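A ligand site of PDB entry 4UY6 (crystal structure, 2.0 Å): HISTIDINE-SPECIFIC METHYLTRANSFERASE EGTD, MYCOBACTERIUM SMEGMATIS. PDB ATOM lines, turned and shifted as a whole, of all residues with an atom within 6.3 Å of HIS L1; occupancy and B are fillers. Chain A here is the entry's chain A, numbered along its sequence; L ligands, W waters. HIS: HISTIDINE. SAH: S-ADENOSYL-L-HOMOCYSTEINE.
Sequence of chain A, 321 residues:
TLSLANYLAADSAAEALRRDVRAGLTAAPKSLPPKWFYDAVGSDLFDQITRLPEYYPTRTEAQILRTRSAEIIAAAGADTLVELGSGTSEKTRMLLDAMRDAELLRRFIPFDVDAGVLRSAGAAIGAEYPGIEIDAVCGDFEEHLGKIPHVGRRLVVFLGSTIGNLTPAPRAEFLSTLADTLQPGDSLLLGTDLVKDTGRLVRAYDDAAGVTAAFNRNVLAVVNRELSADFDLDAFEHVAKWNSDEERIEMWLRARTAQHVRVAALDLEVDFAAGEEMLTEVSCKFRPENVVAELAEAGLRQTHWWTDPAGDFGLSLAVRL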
ATOM      1  N   PHE A  37      10.157  10.709  12.012  1.00  0.00           N
ATOM      2  CA  PHE A  37      11.518  10.741  12.531  1.00  0.00           C
ATOM      3  C   PHE A  37      12.187  12.058  12.187  1.00  0.00           C
ATOM      4  O   PHE A  37      13.076  12.535  12.886  1.00  0.00           O
ATOM      5  CB  PHE A  37      12.367   9.610  11.941  1.00  0.00           C
ATOM      6  CG  PHE A  37      12.076   8.255  12.507  1.00  0.00           C
ATOM      7  CD1 PHE A  37      11.977   8.051  13.870  1.00  0.00           C
ATOM      8  CD2 PHE A  37      11.905   7.167  11.648  1.00  0.00           C
ATOM      9  CE1 PHE A  37      11.721   6.799  14.370  1.00  0.00           C
ATOM     10  CE2 PHE A  37      11.643   5.907  12.149  1.00  0.00           C
ATOM     11  CZ  PHE A  37      11.552   5.711  13.520  1.00  0.00           C
ATOM     12  N   TYR A  38      11.755  12.658  11.075  1.00  0.00           N
ATOM     13  CA  TYR A  38      12.589  13.663  10.429  1.00  0.00           C
ATOM     14  C   TYR A  38      12.143  15.121  10.611  1.00  0.00           C
ATOM     15  O   TYR A  38      11.778  15.800   9.651  1.00  0.00           O
ATOM     16  CB  TYR A  38      12.686  13.310   8.942  1.00  0.00           C
ATOM     17  CG  TYR A  38      13.227  11.906   8.735  1.00  0.00           C
ATOM     18  CD1 TYR A  38      14.588  11.668   8.756  1.00  0.00           C
ATOM     19  CD2 TYR A  38      12.363  10.824   8.555  1.00  0.00           C
ATOM     20  CE1 TYR A  38      15.087  10.392   8.577  1.00  0.00           C
ATOM     21  CE2 TYR A  38      12.853   9.554   8.377  1.00  0.00           C
ATOM     22  CZ  TYR A  38      14.223   9.347   8.397  1.00  0.00           C
ATOM     23  OH  TYR A  38      14.734   8.087   8.226  1.00  0.00           O
ATOM     24  N   PHE A  46      19.926  11.016  11.979  1.00  0.00           N
ATOM     25  CA  PHE A  46      20.148  10.074  10.884  1.00  0.00           C
ATOM     26  C   PHE A  46      21.534  10.302  10.306  1.00  0.00           C
ATOM     27  O   PHE A  46      22.244   9.360   9.932  1.00  0.00           O
ATOM     28  CB  PHE A  46      19.129  10.199   9.774  1.00  0.00           C
ATOM     29  CG  PHE A  46      19.501   9.375   8.574  1.00  0.00           C
ATOM     30  CD1 PHE A  46      19.329   8.004   8.594  1.00  0.00           C
ATOM     31  CD2 PHE A  46      20.077   9.961   7.461  1.00  0.00           C
ATOM     32  CE1 PHE A  46      19.697   7.219   7.507  1.00  0.00           C
ATOM     33  CE2 PHE A  46      20.447   9.198   6.363  1.00  0.00           C
ATOM     34  CZ  PHE A  46      20.261   7.824   6.385  1.00  0.00           C
ATOM     35  N   ILE A  49      23.878   8.522  12.246  1.00  0.00           N
ATOM     36  CA  ILE A  49      23.791   7.081  12.039  1.00  0.00           C
ATOM     37  C   ILE A  49      24.652   6.679  10.843  1.00  0.00           C
ATOM     38  O   ILE A  49      25.333   5.645  10.899  1.00  0.00           O
ATOM     39  CB  ILE A  49      22.309   6.606  11.821  1.00  0.00           C
ATOM     40  CG1 ILE A  49      21.583   6.582  13.164  1.00  0.00           C
ATOM     41  CG2 ILE A  49      22.257   5.217  11.163  1.00  0.00           C
ATOM     42  CD1 ILE A  49      20.108   6.305  13.047  1.00  0.00           C
ATOM     43  N   TYR A  55      26.572   0.710  10.842  1.00  0.00           N
ATOM     44  CA  TYR A  55      25.684   1.074   9.742  1.00  0.00           C
ATOM     45  C   TYR A  55      26.434   1.095   8.405  1.00  0.00           C
ATOM     46  O   TYR A  55      26.837   2.152   7.910  1.00  0.00           O
ATOM     47  CB  TYR A  55      25.016   2.423  10.000  1.00  0.00           C
ATOM     48  CG  TYR A  55      23.814   2.671   9.123  1.00  0.00           C
ATOM     49  CD1 TYR A  55      22.617   1.988   9.343  1.00  0.00           C
ATOM     50  CD2 TYR A  55      23.881   3.556   8.053  1.00  0.00           C
ATOM     51  CE1 TYR A  55      21.505   2.207   8.532  1.00  0.00           C
ATOM     52  CE2 TYR A  55      22.790   3.772   7.238  1.00  0.00           C
ATOM     53  CZ  TYR A  55      21.602   3.097   7.478  1.00  0.00           C
ATOM     54  OH  TYR A  55      20.525   3.315   6.661  1.00  0.00           O
ATOM     55  N   PRO A  57      25.194   0.581   5.300  1.00  0.00           N
ATOM     56  CA  PRO A  57      24.608   1.014   4.030  1.00  0.00           C
ATOM     57  C   PRO A  57      25.149   2.316   3.413  1.00  0.00           C
ATOM     58  O   PRO A  57      25.338   2.352   2.187  1.00  0.00           O
ATOM     59  CB  PRO A  57      23.125   1.202   4.373  1.00  0.00           C
ATOM     60  CG  PRO A  57      22.885   0.214   5.420  1.00  0.00           C
ATOM     61  CD  PRO A  57      24.129   0.212   6.261  1.00  0.00           C
ATOM     62  N   GLY A 160      19.886   5.123  -0.499  1.00  0.00           N
ATOM     63  CA  GLY A 160      19.909   4.781   0.914  1.00  0.00           C
ATOM     64  C   GLY A 160      18.937   3.715   1.349  1.00  0.00           C
ATOM     65  O   GLY A 160      18.707   3.536   2.560  1.00  0.00           O
ATOM     66  N   SER A 161      18.357   3.002   0.385  1.00  0.00           N
ATOM     67  CA  SER A 161      17.359   1.972   0.663  1.00  0.00           C
ATOM     68  C   SER A 161      16.153   2.527   1.439  1.00  0.00           C
ATOM     69  O   SER A 161      15.478   1.800   2.173  1.00  0.00           O
ATOM     70  CB  SER A 161      17.965   0.797   1.449  1.00  0.00           C
ATOM     71  OG  SER A 161      17.187  -0.369   1.255  1.00  0.00           O
ATOM     72  N   THR A 162      15.861   3.805   1.230  1.00  0.00           N
ATOM     73  CA  THR A 162      14.654   4.388   1.804  1.00  0.00           C
ATOM     74  C   THR A 162      13.419   3.689   1.271  1.00  0.00           C
ATOM     75  O   THR A 162      12.384   3.646   1.945  1.00  0.00           O
ATOM     76  CB  THR A 162      14.580   5.910   1.521  1.00  0.00           C
ATOM     77  OG1 THR A 162      15.792   6.515   1.936  1.00  0.00           O
ATOM     78  CG2 THR A 162      13.396   6.570   2.284  1.00  0.00           C
ATOM     79  N   GLY A 164      12.885   0.750   1.209  1.00  0.00           N
ATOM     80  CA  GLY A 164      12.623  -0.360   2.117  1.00  0.00           C
ATOM     81  C   GLY A 164      11.895   0.057   3.382  1.00  0.00           C
ATOM     82  O   GLY A 164      11.488  -0.810   4.173  1.00  0.00           O
ATOM     83  N   ASN A 165      11.703   1.368   3.563  1.00  0.00           N
ATOM     84  CA  ASN A 165      10.932   1.861   4.704  1.00  0.00           C
ATOM     85  C   ASN A 165       9.422   1.843   4.401  1.00  0.00           C
ATOM     86  O   ASN A 165       8.620   2.241   5.233  1.00  0.00           O
ATOM     87  CB  ASN A 165      11.385   3.268   5.114  1.00  0.00           C
ATOM     88  CG  ASN A 165      12.829   3.302   5.610  1.00  0.00           C
ATOM     89  OD1 ASN A 165      13.575   4.248   5.342  1.00  0.00           O
ATOM     90  ND2 ASN A 165      13.237   2.252   6.307  1.00  0.00           N
ATOM     91  N   ASP A 193      19.228  -2.094  -0.109  1.00  0.00           N
ATOM     92  CA  ASP A 193      20.070  -2.898   0.773  1.00  0.00           C
ATOM     93  C   ASP A 193      19.677  -4.346   0.595  1.00  0.00           C
ATOM     94  O   ASP A 193      18.502  -4.650   0.409  1.00  0.00           O
ATOM     95  CB  ASP A 193      19.903  -2.441   2.221  1.00  0.00           C
ATOM     96  CG  ASP A 193      20.980  -2.964   3.127  1.00  0.00           C
ATOM     97  OD1 ASP A 193      21.967  -3.526   2.619  1.00  0.00           O
ATOM     98  OD2 ASP A 193      20.840  -2.826   4.366  1.00  0.00           O
ATOM     99  N   ALA A 204      23.241  -3.133  12.708  1.00  0.00           N
ATOM    100  CA  ALA A 204      23.184  -1.846  12.025  1.00  0.00           C
ATOM    101  C   ALA A 204      22.015  -0.971  12.504  1.00  0.00           C
ATOM    102  O   ALA A 204      21.968   0.232  12.235  1.00  0.00           O
ATOM    103  CB  ALA A 204      23.089  -2.069  10.540  1.00  0.00           C
ATOM    104  N   TYR A 205      21.057  -1.584  13.203  1.00  0.00           N
ATOM    105  CA  TYR A 205      19.931  -0.840  13.744  1.00  0.00           C
ATOM    106  C   TYR A 205      19.913  -0.912  15.266  1.00  0.00           C
ATOM    107  O   TYR A 205      18.929  -0.557  15.914  1.00  0.00           O
ATOM    108  CB  TYR A 205      18.622  -1.363  13.143  1.00  0.00           C
ATOM    109  CG  TYR A 205      18.558  -1.099  11.656  1.00  0.00           C
ATOM    110  CD1 TYR A 205      19.164  -1.954  10.742  1.00  0.00           C
ATOM    111  CD2 TYR A 205      17.930   0.025  11.176  1.00  0.00           C
ATOM    112  CE1 TYR A 205      19.131  -1.710   9.381  1.00  0.00           C
ATOM    113  CE2 TYR A 205      17.893   0.283   9.806  1.00  0.00           C
ATOM    114  CZ  TYR A 205      18.492  -0.588   8.914  1.00  0.00           C
ATOM    115  OH  TYR A 205      18.459  -0.344   7.553  1.00  0.00           O
ATOM    116  N   THR A 212      21.002   4.892  17.149  1.00  0.00           N
ATOM    117  CA  THR A 212      19.749   4.452  16.539  1.00  0.00           C
ATOM    118  C   THR A 212      18.615   4.500  17.564  1.00  0.00           C
ATOM    119  O   THR A 212      17.485   4.864  17.223  1.00  0.00           O
ATOM    120  CB  THR A 212      19.845   3.030  15.948  1.00  0.00           C
ATOM    121  OG1 THR A 212      20.991   2.942  15.083  1.00  0.00           O
ATOM    122  CG2 THR A 212      18.587   2.704  15.127  1.00  0.00           C
ATOM    123  N   PHE A 215      17.518   8.007  17.854  1.00  0.00           N
ATOM    124  CA  PHE A 215      16.801   8.328  16.635  1.00  0.00           C
ATOM    125  C   PHE A 215      15.380   7.754  16.679  1.00  0.00           C
ATOM    126  O   PHE A 215      14.407   8.421  16.314  1.00  0.00           O
ATOM    127  CB  PHE A 215      17.566   7.807  15.424  1.00  0.00           C
ATOM    128  CG  PHE A 215      16.867   7.998  14.120  1.00  0.00           C
ATOM    129  CD1 PHE A 215      16.831   9.244  13.515  1.00  0.00           C
ATOM    130  CD2 PHE A 215      16.295   6.923  13.457  1.00  0.00           C
ATOM    131  CE1 PHE A 215      16.199   9.422  12.291  1.00  0.00           C
ATOM    132  CE2 PHE A 215      15.666   7.088  12.232  1.00  0.00           C
ATOM    133  CZ  PHE A 215      15.617   8.330  11.640  1.00  0.00           C
ATOM    134  N   MET A 251      12.105  -1.710  13.631  1.00  0.00           N
ATOM    135  CA  MET A 251      12.378  -0.969  14.847  1.00  0.00           C
ATOM    136  C   MET A 251      11.077  -0.835  15.616  1.00  0.00           C
ATOM    137  O   MET A 251      10.028  -0.476  15.049  1.00  0.00           O
ATOM    138  CB  MET A 251      12.978   0.412  14.555  1.00  0.00           C
ATOM    139  CG  MET A 251      14.364   0.381  13.935  1.00  0.00           C
ATOM    140  SD  MET A 251      15.230   1.965  14.178  1.00  0.00           S
ATOM    141  CE  MET A 251      14.005   3.160  13.644  1.00  0.00           C
ATOM    142  N   GLU A 281       9.437   1.734  12.554  1.00  0.00           N
ATOM    143  CA  GLU A 281       9.978   1.689  11.199  1.00  0.00           C
ATOM    144  C   GLU A 281      10.225   0.262  10.725  1.00  0.00           C
ATOM    145  O   GLU A 281      10.633  -0.597  11.515  1.00  0.00           O
ATOM    146  CB  GLU A 281      11.284   2.495  11.124  1.00  0.00           C
ATOM    147  CG  GLU A 281      11.690   2.873   9.702  1.00  0.00           C
ATOM    148  CD  GLU A 281      13.055   3.531   9.637  1.00  0.00           C
ATOM    149  OE1 GLU A 281      14.044   2.913  10.111  1.00  0.00           O
ATOM    150  OE2 GLU A 281      13.141   4.652   9.102  1.00  0.00           O
ATOM    151  N   VAL A 282       9.959   0.007   9.450  1.00  0.00           N
ATOM    152  CA  VAL A 282      10.422  -1.231   8.821  1.00  0.00           C
ATOM    153  C   VAL A 282      11.539  -0.874   7.852  1.00  0.00           C
ATOM    154  O   VAL A 282      11.536   0.218   7.271  1.00  0.00           O
ATOM    155  CB  VAL A 282       9.297  -1.994   8.037  1.00  0.00           C
ATOM    156  CG1 VAL A 282       8.064  -2.232   8.924  1.00  0.00           C
ATOM    157  CG2 VAL A 282       8.900  -1.252   6.768  1.00  0.00           C
ATOM    158  N   SER A 283      12.484  -1.794   7.693  1.00  0.00           N
ATOM    159  CA  SER A 283      13.572  -1.659   6.737  1.00  0.00           C
ATOM    160  C   SER A 283      13.689  -2.984   5.941  1.00  0.00           C
ATOM    161  O   SER A 283      14.416  -3.906   6.324  1.00  0.00           O
ATOM    162  CB  SER A 283      14.875  -1.336   7.470  1.00  0.00           C
ATOM    163  OG  SER A 283      15.913  -0.954   6.584  1.00  0.00           O
ATOM    164  N   CYS A 284      12.946  -3.068   4.845  1.00  0.00           N
ATOM    165  CA  CYS A 284      12.913  -4.268   4.033  1.00  0.00           C
ATOM    166  C   CYS A 284      14.272  -4.503   3.365  1.00  0.00           C
ATOM    167  O   CYS A 284      14.887  -3.566   2.866  1.00  0.00           O
ATOM    168  CB  CYS A 284      11.773  -4.176   2.993  1.00  0.00           C
ATOM    169  SG  CYS A 284      10.058  -4.017   3.758  1.00  0.00           S
ATOM    170  N   LYS A 285      14.746  -5.741   3.393  1.00  0.00           N
ATOM    171  CA  LYS A 285      15.989  -6.127   2.733  1.00  0.00           C
ATOM    172  C   LYS A 285      15.632  -6.970   1.510  1.00  0.00           C
ATOM    173  O   LYS A 285      14.741  -7.814   1.589  1.00  0.00           O
ATOM    174  CB  LYS A 285      16.906  -6.877   3.694  1.00  0.00           C
ATOM    175  CG  LYS A 285      17.218  -6.095   4.975  1.00  0.00           C
ATOM    176  CD  LYS A 285      17.746  -4.682   4.635  1.00  0.00           C
ATOM    177  CE  LYS A 285      17.829  -3.798   5.882  1.00  0.00           C
ATOM    178  NZ  LYS A 285      18.399  -2.444   5.595  1.00  0.00           N
HETATM  179  N   HIS L   1      16.357   4.714   5.522  1.00  0.00           N
HETATM  180  CA  HIS L   1      17.148   4.237   6.657  1.00  0.00           C
HETATM  181  C   HIS L   1      17.143   2.709   6.710  1.00  0.00           C
HETATM  182  O   HIS L   1      18.166   2.069   6.966  1.00  0.00           O
HETATM  183  CB  HIS L   1      16.606   4.824   7.964  1.00  0.00           C
HETATM  184  CG  HIS L   1      17.272   4.284   9.200  1.00  0.00           C
HETATM  185  ND1 HIS L   1      16.559   3.875  10.306  1.00  0.00           N
HETATM  186  CD2 HIS L   1      18.582   4.085   9.493  1.00  0.00           C
HETATM  187  CE1 HIS L   1      17.393   3.457  11.232  1.00  0.00           C
HETATM  188  NE2 HIS L   1      18.632   3.566  10.769  1.00  0.00           N
HETATM  189  OXT HIS L   1      16.104   2.078   6.480  1.00  0.00           O
HETATM  190  N   SAH L   2      18.880  10.371   1.062  1.00  0.00           N
HETATM  191  CA  SAH L   2      19.672  10.460   2.282  1.00  0.00           C
HETATM  192  CB  SAH L   2      18.778  10.501   3.521  1.00  0.00           C
HETATM  193  CG  SAH L   2      17.939   9.241   3.650  1.00  0.00           C
HETATM  194  SD  SAH L   2      17.053   9.106   5.231  1.00  0.00           S
HETATM  195  C   SAH L   2      20.585   9.245   2.349  1.00  0.00           C
HETATM  196  O   SAH L   2      21.421   9.137   3.247  1.00  0.00           O
HETATM  197  OXT SAH L   2      20.498   8.345   1.507  1.00  0.00           O
HETATM  198  C5' SAH L   2      15.454   9.372   4.398  1.00  0.00           C
HETATM  199  C4' SAH L   2      15.218  10.814   3.918  1.00  0.00           C
HETATM  200  O4' SAH L   2      13.896  10.912   3.383  1.00  0.00           O
HETATM  201  C3' SAH L   2      15.275  11.813   5.049  1.00  0.00           C
HETATM  202  O3' SAH L   2      15.877  12.992   4.573  1.00  0.00           O
HETATM  203  C2' SAH L   2      13.805  12.090   5.390  1.00  0.00           C
HETATM  204  O2' SAH L   2      13.649  13.396   5.879  1.00  0.00           O
HETATM  205  C1' SAH L   2      13.101  11.870   4.065  1.00  0.00           C
HETATM  206  N9  SAH L   2      11.743  11.278   4.119  1.00  0.00           N
HETATM  207  C8  SAH L   2      11.274  10.249   4.919  1.00  0.00           C
HETATM  208  N7  SAH L   2       9.979   9.999   4.591  1.00  0.00           N
HETATM  209  C5  SAH L   2       9.628  10.848   3.599  1.00  0.00           C
HETATM  210  C6  SAH L   2       8.443  11.028   2.880  1.00  0.00           C
HETATM  211  N6  SAH L   2       7.376  10.288   3.161  1.00  0.00           N
HETATM  212  N1  SAH L   2       8.393  11.989   1.901  1.00  0.00           N
HETATM  213  C2  SAH L   2       9.478  12.776   1.608  1.00  0.00           C
HETATM  214  N3  SAH L   2      10.643  12.585   2.320  1.00  0.00           N
HETATM  215  C4  SAH L   2      10.717  11.643   3.295  1.00  0.00           C
HETATM  216  O   HOH W   1      20.531   2.519  12.450  1.00  0.00           O
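Merely in contact with HIS L1: Tyr 38 (3.8 Å), Phe 46 (3.9 Å), Ile 49 (3.9 Å), Gly 160 (3.96 Å), Phe 215 (3.9 Å) and Met 251 (3.9 Å). Hydrophobic or aromatic side chains that line HIS L1: Phe 46, Ile 49, Tyr 55, Tyr 205, Phe 215 and Met 251.
Water W1 lies within hydrogen-bond range of OG1 of Thr 212 (2.7 Å), O of Ala 204 (2.7 Å) and NE2 of HIS L1 (2.7 Å).
The side-chain hydroxyl (OG) of Ser 283 is in hydrogen-bond range of an oxygen (OXT) of HIS L1 (3.0 Å). ND1 of HIS L1 sits at hydrogen-bond distance from OE1 of Glu 281, at 2.7 Å. The side-chain hydroxyl (OH) of Tyr 55 sits at hydrogen-bond distance from an oxygen (O) of HIS L1 (2.7 Å). The side-chain hydroxyl (OH) of Tyr 205 is in hydrogen-bond range of an oxygen (O) of HIS L1, at 2.5 Å. The side-chain amide oxygen of Asn 165 is in hydrogen-bond range of a nitrogen (N) of HIS L1 (2.8 Å).
The side-chain hydroxyl of Ser 283 sits at hydrogen-bond distance from the side-chain amino group of Lys 285 (3.1 Å). O of Glu 281 sits at hydrogen-bond distance from N of Met 251 (2.8 Å). OH of Tyr 205 sits at hydrogen-bond distance from NZ of Lys 285 (2.9 Å). O of Val 282 is in hydrogen-bond range of ND2 of Asn 165, 2.8 Å away. The side-chain hydroxyl of Ser 283 is in hydrogen-bond range of the side-chain hydroxyl of Tyr 205 (2.8 Å).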
